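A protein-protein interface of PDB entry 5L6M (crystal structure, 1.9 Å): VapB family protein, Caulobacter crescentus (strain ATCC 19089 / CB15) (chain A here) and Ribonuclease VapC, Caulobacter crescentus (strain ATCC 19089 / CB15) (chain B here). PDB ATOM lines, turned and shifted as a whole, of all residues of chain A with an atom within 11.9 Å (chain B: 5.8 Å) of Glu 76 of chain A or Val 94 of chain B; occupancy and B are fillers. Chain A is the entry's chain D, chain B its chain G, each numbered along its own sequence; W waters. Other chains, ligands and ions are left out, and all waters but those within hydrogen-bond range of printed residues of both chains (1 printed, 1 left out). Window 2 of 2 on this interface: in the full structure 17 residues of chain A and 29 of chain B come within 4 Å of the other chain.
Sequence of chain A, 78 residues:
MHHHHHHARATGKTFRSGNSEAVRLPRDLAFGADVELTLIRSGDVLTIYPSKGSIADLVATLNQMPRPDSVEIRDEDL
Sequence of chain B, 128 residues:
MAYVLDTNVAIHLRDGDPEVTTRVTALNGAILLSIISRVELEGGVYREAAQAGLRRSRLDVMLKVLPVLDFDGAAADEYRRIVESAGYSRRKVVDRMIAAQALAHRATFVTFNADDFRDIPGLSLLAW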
ATOM      1  N   GLU A  72       3.445   2.478  25.607  1.00  0.00           N
ATOM      2  CA  GLU A  72       2.628   1.676  24.710  1.00  0.00           C
ATOM      3  C   GLU A  72       1.925   2.552  23.692  1.00  0.00           C
ATOM      4  O   GLU A  72       1.567   3.698  23.972  1.00  0.00           O
ATOM      5  CB  GLU A  72       1.590   0.884  25.504  1.00  0.00           C
ATOM      6  CG  GLU A  72       2.002  -0.527  25.694  1.00  0.00           C
ATOM      7  CD  GLU A  72       0.981  -1.317  26.468  1.00  0.00           C
ATOM      8  OE1 GLU A  72      -0.123  -0.790  26.711  1.00  0.00           O
ATOM      9  OE2 GLU A  72       1.314  -2.451  26.848  1.00  0.00           O
ATOM     10  N   ILE A  73       1.728   1.999  22.499  1.00  0.00           N
ATOM     11  CA  ILE A  73       0.937   2.674  21.483  1.00  0.00           C
ATOM     12  C   ILE A  73      -0.542   2.365  21.700  1.00  0.00           C
ATOM     13  O   ILE A  73      -0.908   1.250  22.091  1.00  0.00           O
ATOM     14  CB  ILE A  73       1.434   2.243  20.098  1.00  0.00           C
ATOM     15  CG1 ILE A  73       2.835   2.827  19.870  1.00  0.00           C
ATOM     16  CG2 ILE A  73       0.476   2.681  19.016  1.00  0.00           C
ATOM     17  CD1 ILE A  73       3.653   2.032  18.899  1.00  0.00           C
ATOM     18  N   ARG A  74      -1.403   3.361  21.491  1.00  0.00           N
ATOM     19  CA  ARG A  74      -2.844   3.154  21.645  1.00  0.00           C
ATOM     20  C   ARG A  74      -3.377   2.360  20.458  1.00  0.00           C
ATOM     21  O   ARG A  74      -3.452   2.874  19.334  1.00  0.00           O
ATOM     22  CB  ARG A  74      -3.573   4.484  21.756  1.00  0.00           C
ATOM     23  CG  ARG A  74      -5.071   4.317  21.832  1.00  0.00           C
ATOM     24  CD  ARG A  74      -5.737   5.621  22.116  1.00  0.00           C
ATOM     25  NE  ARG A  74      -7.160   5.446  22.433  1.00  0.00           N
ATOM     26  CZ  ARG A  74      -8.155   5.975  21.735  1.00  0.00           C
ATOM     27  NH1 ARG A  74      -7.884   6.738  20.687  1.00  0.00           N
ATOM     28  NH2 ARG A  74      -9.415   5.768  22.098  1.00  0.00           N
ATOM     29  N   ASP A  75      -3.763   1.109  20.703  1.00  0.00           N
ATOM     30  CA  ASP A  75      -4.129   0.227  19.599  1.00  0.00           C
ATOM     31  C   ASP A  75      -5.385   0.709  18.877  1.00  0.00           C
ATOM     32  O   ASP A  75      -5.546   0.469  17.671  1.00  0.00           O
ATOM     33  CB  ASP A  75      -4.294  -1.199  20.131  1.00  0.00           C
ATOM     34  CG  ASP A  75      -4.101  -2.255  19.055  1.00  0.00           C
ATOM     35  OD1 ASP A  75      -3.234  -2.081  18.169  1.00  0.00           O
ATOM     36  OD2 ASP A  75      -4.824  -3.266  19.098  1.00  0.00           O
ATOM     37  N   GLU A  76      -6.249   1.454  19.563  1.00  0.00           N
ATOM     38  CA  GLU A  76      -7.485   1.884  18.917  1.00  0.00           C
ATOM     39  C   GLU A  76      -7.215   2.843  17.757  1.00  0.00           C
ATOM     40  O   GLU A  76      -7.999   2.893  16.802  1.00  0.00           O
ATOM     41  CB  GLU A  76      -8.417   2.513  19.961  1.00  0.00           C
ATOM     42  CG  GLU A  76      -9.801   2.857  19.438  1.00  0.00           C
ATOM     43  CD  GLU A  76     -10.659   1.621  19.217  1.00  0.00           C
ATOM     44  OE1 GLU A  76     -11.566   1.688  18.368  1.00  0.00           O
ATOM     45  OE2 GLU A  76     -10.419   0.586  19.892  1.00  0.00           O
ATOM     46  N   ASP A  77      -6.109   3.596  17.798  1.00  0.00           N
ATOM     47  CA  ASP A  77      -5.856   4.583  16.748  1.00  0.00           C
ATOM     48  C   ASP A  77      -5.435   3.936  15.434  1.00  0.00           C
ATOM     49  O   ASP A  77      -5.627   4.533  14.370  1.00  0.00           O
ATOM     50  CB  ASP A  77      -4.778   5.581  17.190  1.00  0.00           C
ATOM     51  CG  ASP A  77      -5.255   6.520  18.291  1.00  0.00           C
ATOM     52  OD1 ASP A  77      -6.475   6.733  18.405  1.00  0.00           O
ATOM     53  OD2 ASP A  77      -4.416   7.027  19.064  1.00  0.00           O
ATOM     54  N   LEU A  78      -4.875   2.733  15.483  1.00  0.00           N
ATOM     55  CA  LEU A  78      -4.395   2.063  14.282  1.00  0.00           C
ATOM     56  C   LEU A  78      -5.540   1.450  13.484  1.00  0.00           C
ATOM     57  O   LEU A  78      -5.571   1.575  12.262  1.00  0.00           O
ATOM     58  CB  LEU A  78      -3.368   0.996  14.656  1.00  0.00           C
ATOM     59  CG  LEU A  78      -2.194   1.570  15.455  1.00  0.00           C
ATOM     60  CD1 LEU A  78      -1.314   0.464  16.026  1.00  0.00           C
ATOM     61  CD2 LEU A  78      -1.384   2.523  14.572  1.00  0.00           C
ATOM     62  N   ILE B  36     -14.178   3.967  29.501  1.00  0.00           N
ATOM     63  CA  ILE B  36     -13.700   3.445  28.225  1.00  0.00           C
ATOM     64  C   ILE B  36     -12.170   3.442  28.202  1.00  0.00           C
ATOM     65  O   ILE B  36     -11.540   2.471  27.779  1.00  0.00           O
ATOM     66  CB  ILE B  36     -14.299   4.254  27.057  1.00  0.00           C
ATOM     67  CG1 ILE B  36     -15.826   4.271  27.136  1.00  0.00           C
ATOM     68  CG2 ILE B  36     -13.888   3.667  25.710  1.00  0.00           C
ATOM     69  CD1 ILE B  36     -16.433   2.897  27.405  1.00  0.00           C
ATOM     70  N   GLU B  40      -9.294   0.285  27.792  1.00  0.00           N
ATOM     71  CA  GLU B  40      -8.127   0.269  26.914  1.00  0.00           C
ATOM     72  C   GLU B  40      -6.854   0.056  27.715  1.00  0.00           C
ATOM     73  O   GLU B  40      -5.978  -0.711  27.308  1.00  0.00           O
ATOM     74  CB  GLU B  40      -8.036   1.587  26.142  1.00  0.00           C
ATOM     75  CG  GLU B  40      -9.205   1.840  25.166  1.00  0.00           C
ATOM     76  CD  GLU B  40      -9.013   3.127  24.390  1.00  0.00           C
ATOM     77  OE1 GLU B  40      -9.593   4.159  24.790  1.00  0.00           O
ATOM     78  OE2 GLU B  40      -8.268   3.099  23.387  1.00  0.00           O
ATOM     79  N   ARG B  90     -17.750   5.379  12.013  1.00  0.00           N
ATOM     80  CA  ARG B  90     -17.396   4.147  12.711  1.00  0.00           C
ATOM     81  C   ARG B  90     -16.056   4.281  13.418  1.00  0.00           C
ATOM     82  O   ARG B  90     -15.912   3.870  14.578  1.00  0.00           O
ATOM     83  CB  ARG B  90     -17.365   2.971  11.738  1.00  0.00           C
ATOM     84  CG  ARG B  90     -17.071   1.633  12.408  1.00  0.00           C
ATOM     85  CD  ARG B  90     -16.601   0.573  11.408  1.00  0.00           C
ATOM     86  NE  ARG B  90     -15.345   0.944  10.753  1.00  0.00           N
ATOM     87  CZ  ARG B  90     -14.132   0.738  11.264  1.00  0.00           C
ATOM     88  NH1 ARG B  90     -13.984   0.156  12.451  1.00  0.00           N
ATOM     89  NH2 ARG B  90     -13.059   1.118  10.581  1.00  0.00           N
ATOM     90  N   ARG B  91     -15.073   4.883  12.747  1.00  0.00           N
ATOM     91  CA  ARG B  91     -13.736   4.982  13.316  1.00  0.00           C
ATOM     92  C   ARG B  91     -13.692   5.846  14.569  1.00  0.00           C
ATOM     93  O   ARG B  91     -12.734   5.736  15.336  1.00  0.00           O
ATOM     94  CB  ARG B  91     -12.749   5.527  12.274  1.00  0.00           C
ATOM     95  CG  ARG B  91     -13.244   6.746  11.493  1.00  0.00           C
ATOM     96  CD  ARG B  91     -12.117   7.454  10.722  1.00  0.00           C
ATOM     97  NE  ARG B  91     -11.420   6.601   9.753  1.00  0.00           N
ATOM     98  CZ  ARG B  91     -11.709   6.533   8.453  1.00  0.00           C
ATOM     99  NH1 ARG B  91     -11.007   5.737   7.655  1.00  0.00           N
ATOM    100  NH2 ARG B  91     -12.701   7.255   7.945  1.00  0.00           N
ATOM    101  N   LYS B  92     -14.693   6.697  14.803  1.00  0.00           N
ATOM    102  CA  LYS B  92     -14.637   7.651  15.906  1.00  0.00           C
ATOM    103  C   LYS B  92     -15.564   7.292  17.063  1.00  0.00           C
ATOM    104  O   LYS B  92     -15.684   8.080  18.008  1.00  0.00           O
ATOM    105  CB  LYS B  92     -14.954   9.062  15.410  1.00  0.00           C
ATOM    106  CG  LYS B  92     -14.122   9.508  14.205  1.00  0.00           C
ATOM    107  CD  LYS B  92     -14.319  10.986  13.889  1.00  0.00           C
ATOM    108  CE  LYS B  92     -13.440  11.852  14.799  1.00  0.00           C
ATOM    109  NZ  LYS B  92     -13.402  13.288  14.394  1.00  0.00           N
ATOM    110  N   VAL B  93     -16.200   6.119  17.027  1.00  0.00           N
ATOM    111  CA  VAL B  93     -17.160   5.755  18.069  1.00  0.00           C
ATOM    112  C   VAL B  93     -16.503   5.766  19.446  1.00  0.00           C
ATOM    113  O   VAL B  93     -16.989   6.414  20.377  1.00  0.00           O
ATOM    114  CB  VAL B  93     -17.790   4.389  17.759  1.00  0.00           C
ATOM    115  CG1 VAL B  93     -18.702   3.969  18.898  1.00  0.00           C
ATOM    116  CG2 VAL B  93     -18.566   4.465  16.445  1.00  0.00           C
ATOM    117  N   VAL B  94     -15.386   5.049  19.591  1.00  0.00           N
ATOM    118  CA  VAL B  94     -14.715   4.961  20.888  1.00  0.00           C
ATOM    119  C   VAL B  94     -14.298   6.342  21.374  1.00  0.00           C
ATOM    120  O   VAL B  94     -14.592   6.733  22.511  1.00  0.00           O
ATOM    121  CB  VAL B  94     -13.513   4.005  20.800  1.00  0.00           C
ATOM    122  CG1 VAL B  94     -12.683   4.016  22.120  1.00  0.00           C
ATOM    123  CG2 VAL B  94     -14.011   2.601  20.478  1.00  0.00           C
ATOM    124  N   ASP B  95     -13.587   7.092  20.526  1.00  0.00           N
ATOM    125  CA  ASP B  95     -13.208   8.464  20.863  1.00  0.00           C
ATOM    126  C   ASP B  95     -14.413   9.298  21.269  1.00  0.00           C
ATOM    127  O   ASP B  95     -14.333  10.099  22.201  1.00  0.00           O
ATOM    128  CB  ASP B  95     -12.496   9.123  19.679  1.00  0.00           C
ATOM    129  CG  ASP B  95     -11.062   8.633  19.510  1.00  0.00           C
ATOM    130  OD1 ASP B  95     -10.633   7.731  20.274  1.00  0.00           O
ATOM    131  OD2 ASP B  95     -10.369   9.149  18.607  1.00  0.00           O
ATOM    132  N   ARG B  96     -15.526   9.163  20.551  1.00  0.00           N
ATOM    133  CA  ARG B  96     -16.694   9.967  20.883  1.00  0.00           C
ATOM    134  C   ARG B  96     -17.364   9.505  22.175  1.00  0.00           C
ATOM    135  O   ARG B  96     -17.974  10.329  22.866  1.00  0.00           O
ATOM    136  CB  ARG B  96     -17.688   9.958  19.722  1.00  0.00           C
ATOM    137  CG  ARG B  96     -17.220  10.841  18.556  1.00  0.00           C
ATOM    138  CD  ARG B  96     -18.060  10.626  17.323  1.00  0.00           C
ATOM    139  NE  ARG B  96     -17.636  11.498  16.228  1.00  0.00           N
ATOM    140  CZ  ARG B  96     -18.288  11.599  15.081  1.00  0.00           C
ATOM    141  NH1 ARG B  96     -19.387  10.878  14.884  1.00  0.00           N
ATOM    142  NH2 ARG B  96     -17.845  12.422  14.136  1.00  0.00           N
ATOM    143  N   MET B  97     -17.273   8.208  22.512  1.00  0.00           N
ATOM    144  CA  MET B  97     -17.756   7.751  23.820  1.00  0.00           C
ATOM    145  C   MET B  97     -16.970   8.396  24.957  1.00  0.00           C
ATOM    146  O   MET B  97     -17.545   8.790  25.980  1.00  0.00           O
ATOM    147  CB  MET B  97     -17.654   6.225  23.938  1.00  0.00           C
ATOM    148  CG  MET B  97     -18.648   5.417  23.064  1.00  0.00           C
ATOM    149  SD  MET B  97     -18.720   3.656  23.544  1.00  0.00           S
ATOM    150  CE  MET B  97     -16.984   3.270  23.774  1.00  0.00           C
ATOM    151  N   ILE B  98     -15.653   8.512  24.795  1.00  0.00           N
ATOM    152  CA  ILE B  98     -14.821   9.138  25.819  1.00  0.00           C
ATOM    153  C   ILE B  98     -15.120  10.629  25.896  1.00  0.00           C
ATOM    154  O   ILE B  98     -15.300  11.179  26.988  1.00  0.00           O
ATOM    155  CB  ILE B  98     -13.335   8.878  25.522  1.00  0.00           C
ATOM    156  CG1 ILE B  98     -13.026   7.372  25.568  1.00  0.00           C
ATOM    157  CG2 ILE B  98     -12.435   9.665  26.484  1.00  0.00           C
ATOM    158  CD1 ILE B  98     -11.777   7.040  24.783  1.00  0.00           C
ATOM    159  N   ALA B  99     -15.227  11.298  24.739  1.00  0.00           N
ATOM    160  CA  ALA B  99     -15.581  12.717  24.750  1.00  0.00           C
ATOM    161  C   ALA B  99     -16.989  12.944  25.302  1.00  0.00           C
ATOM    162  O   ALA B  99     -17.242  13.947  25.984  1.00  0.00           O
ATOM    163  CB  ALA B  99     -15.454  13.311  23.351  1.00  0.00           C
HETATM  164  O   HOH W   1      -6.718   1.255  22.542  1.00  0.00           O
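Ile 73 of chain A touches none of the printed residues of chain B. Of the printed residues of chain B, Arg 74 of chain A touches Glu 40, Val 94, Asp 95 and Ile 98. Glu 76 of chain A touches just these residues of chain B: Glu 40 and Val 94. No residue of chain A comes within 4 Å of Ile 36 of chain B. Of the printed residues of chain A, Glu 40 of chain B touches Arg 74 (2.8 Å) and Glu 76 (3.5 Å). Lys 92 of chain B touches none of the printed residues of chain A. No residue of chain A comes within 4 Å of Val 93 of chain B. Of chain A, only Arg 74 and Glu 76 come within 4 Å of Val 94 of chain B. No residue of chain A comes within 4 Å of Met 97 of chain B. Ile 98 of chain B touches one residue of chain A. The nearest residue of chain A that does not touch Val 94 of chain B is Asp 77 of chain A (7.7 Å). The nearest printed residue of chain B that does not touch Arg 74 of chain A is Ile 36 of chain B (6.1 Å).
The side-chain carboxylate of Asp 77 of chain A lies within salt-bridge range of the guanidinium group of Arg 74 of chain A (2.7 Å).
Of the 7 printed residues of chain A, 2 touch a printed residue of chain B. Of the 12 printed residues of chain B, 4 touch a printed residue of chain A. Printed residues of chain B that touch a printed residue of chain A: Glu 40, Val 94, Asp 95 and Ile 98.
The side-chain carboxylate of Glu 40 of chain B is in salt-bridge range of the guanidinium group of Arg 74 of chain A (2.8 Å). NH2 of Arg 74 of chain A is in salt-bridge range of OD1 of Asp 95 of chain B (2.9 Å).
Val 94 of chain B touches Arg 74 of chain A. Arg 74 of chain A touches Ile 98 of chain B. CB of Glu 76 of chain A touches OE2 of Glu 40 of chain B, 3.5 Å away. Val 94 of chain B touches Glu 76 of chain A.
Water W1 lies within hydrogen-bond range of OE2 of Glu 40 of chain B (2.6 Å), N of Glu 76 of chain A (3.0 Å) and N of Asp 75 of chain A (3.5 Å).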
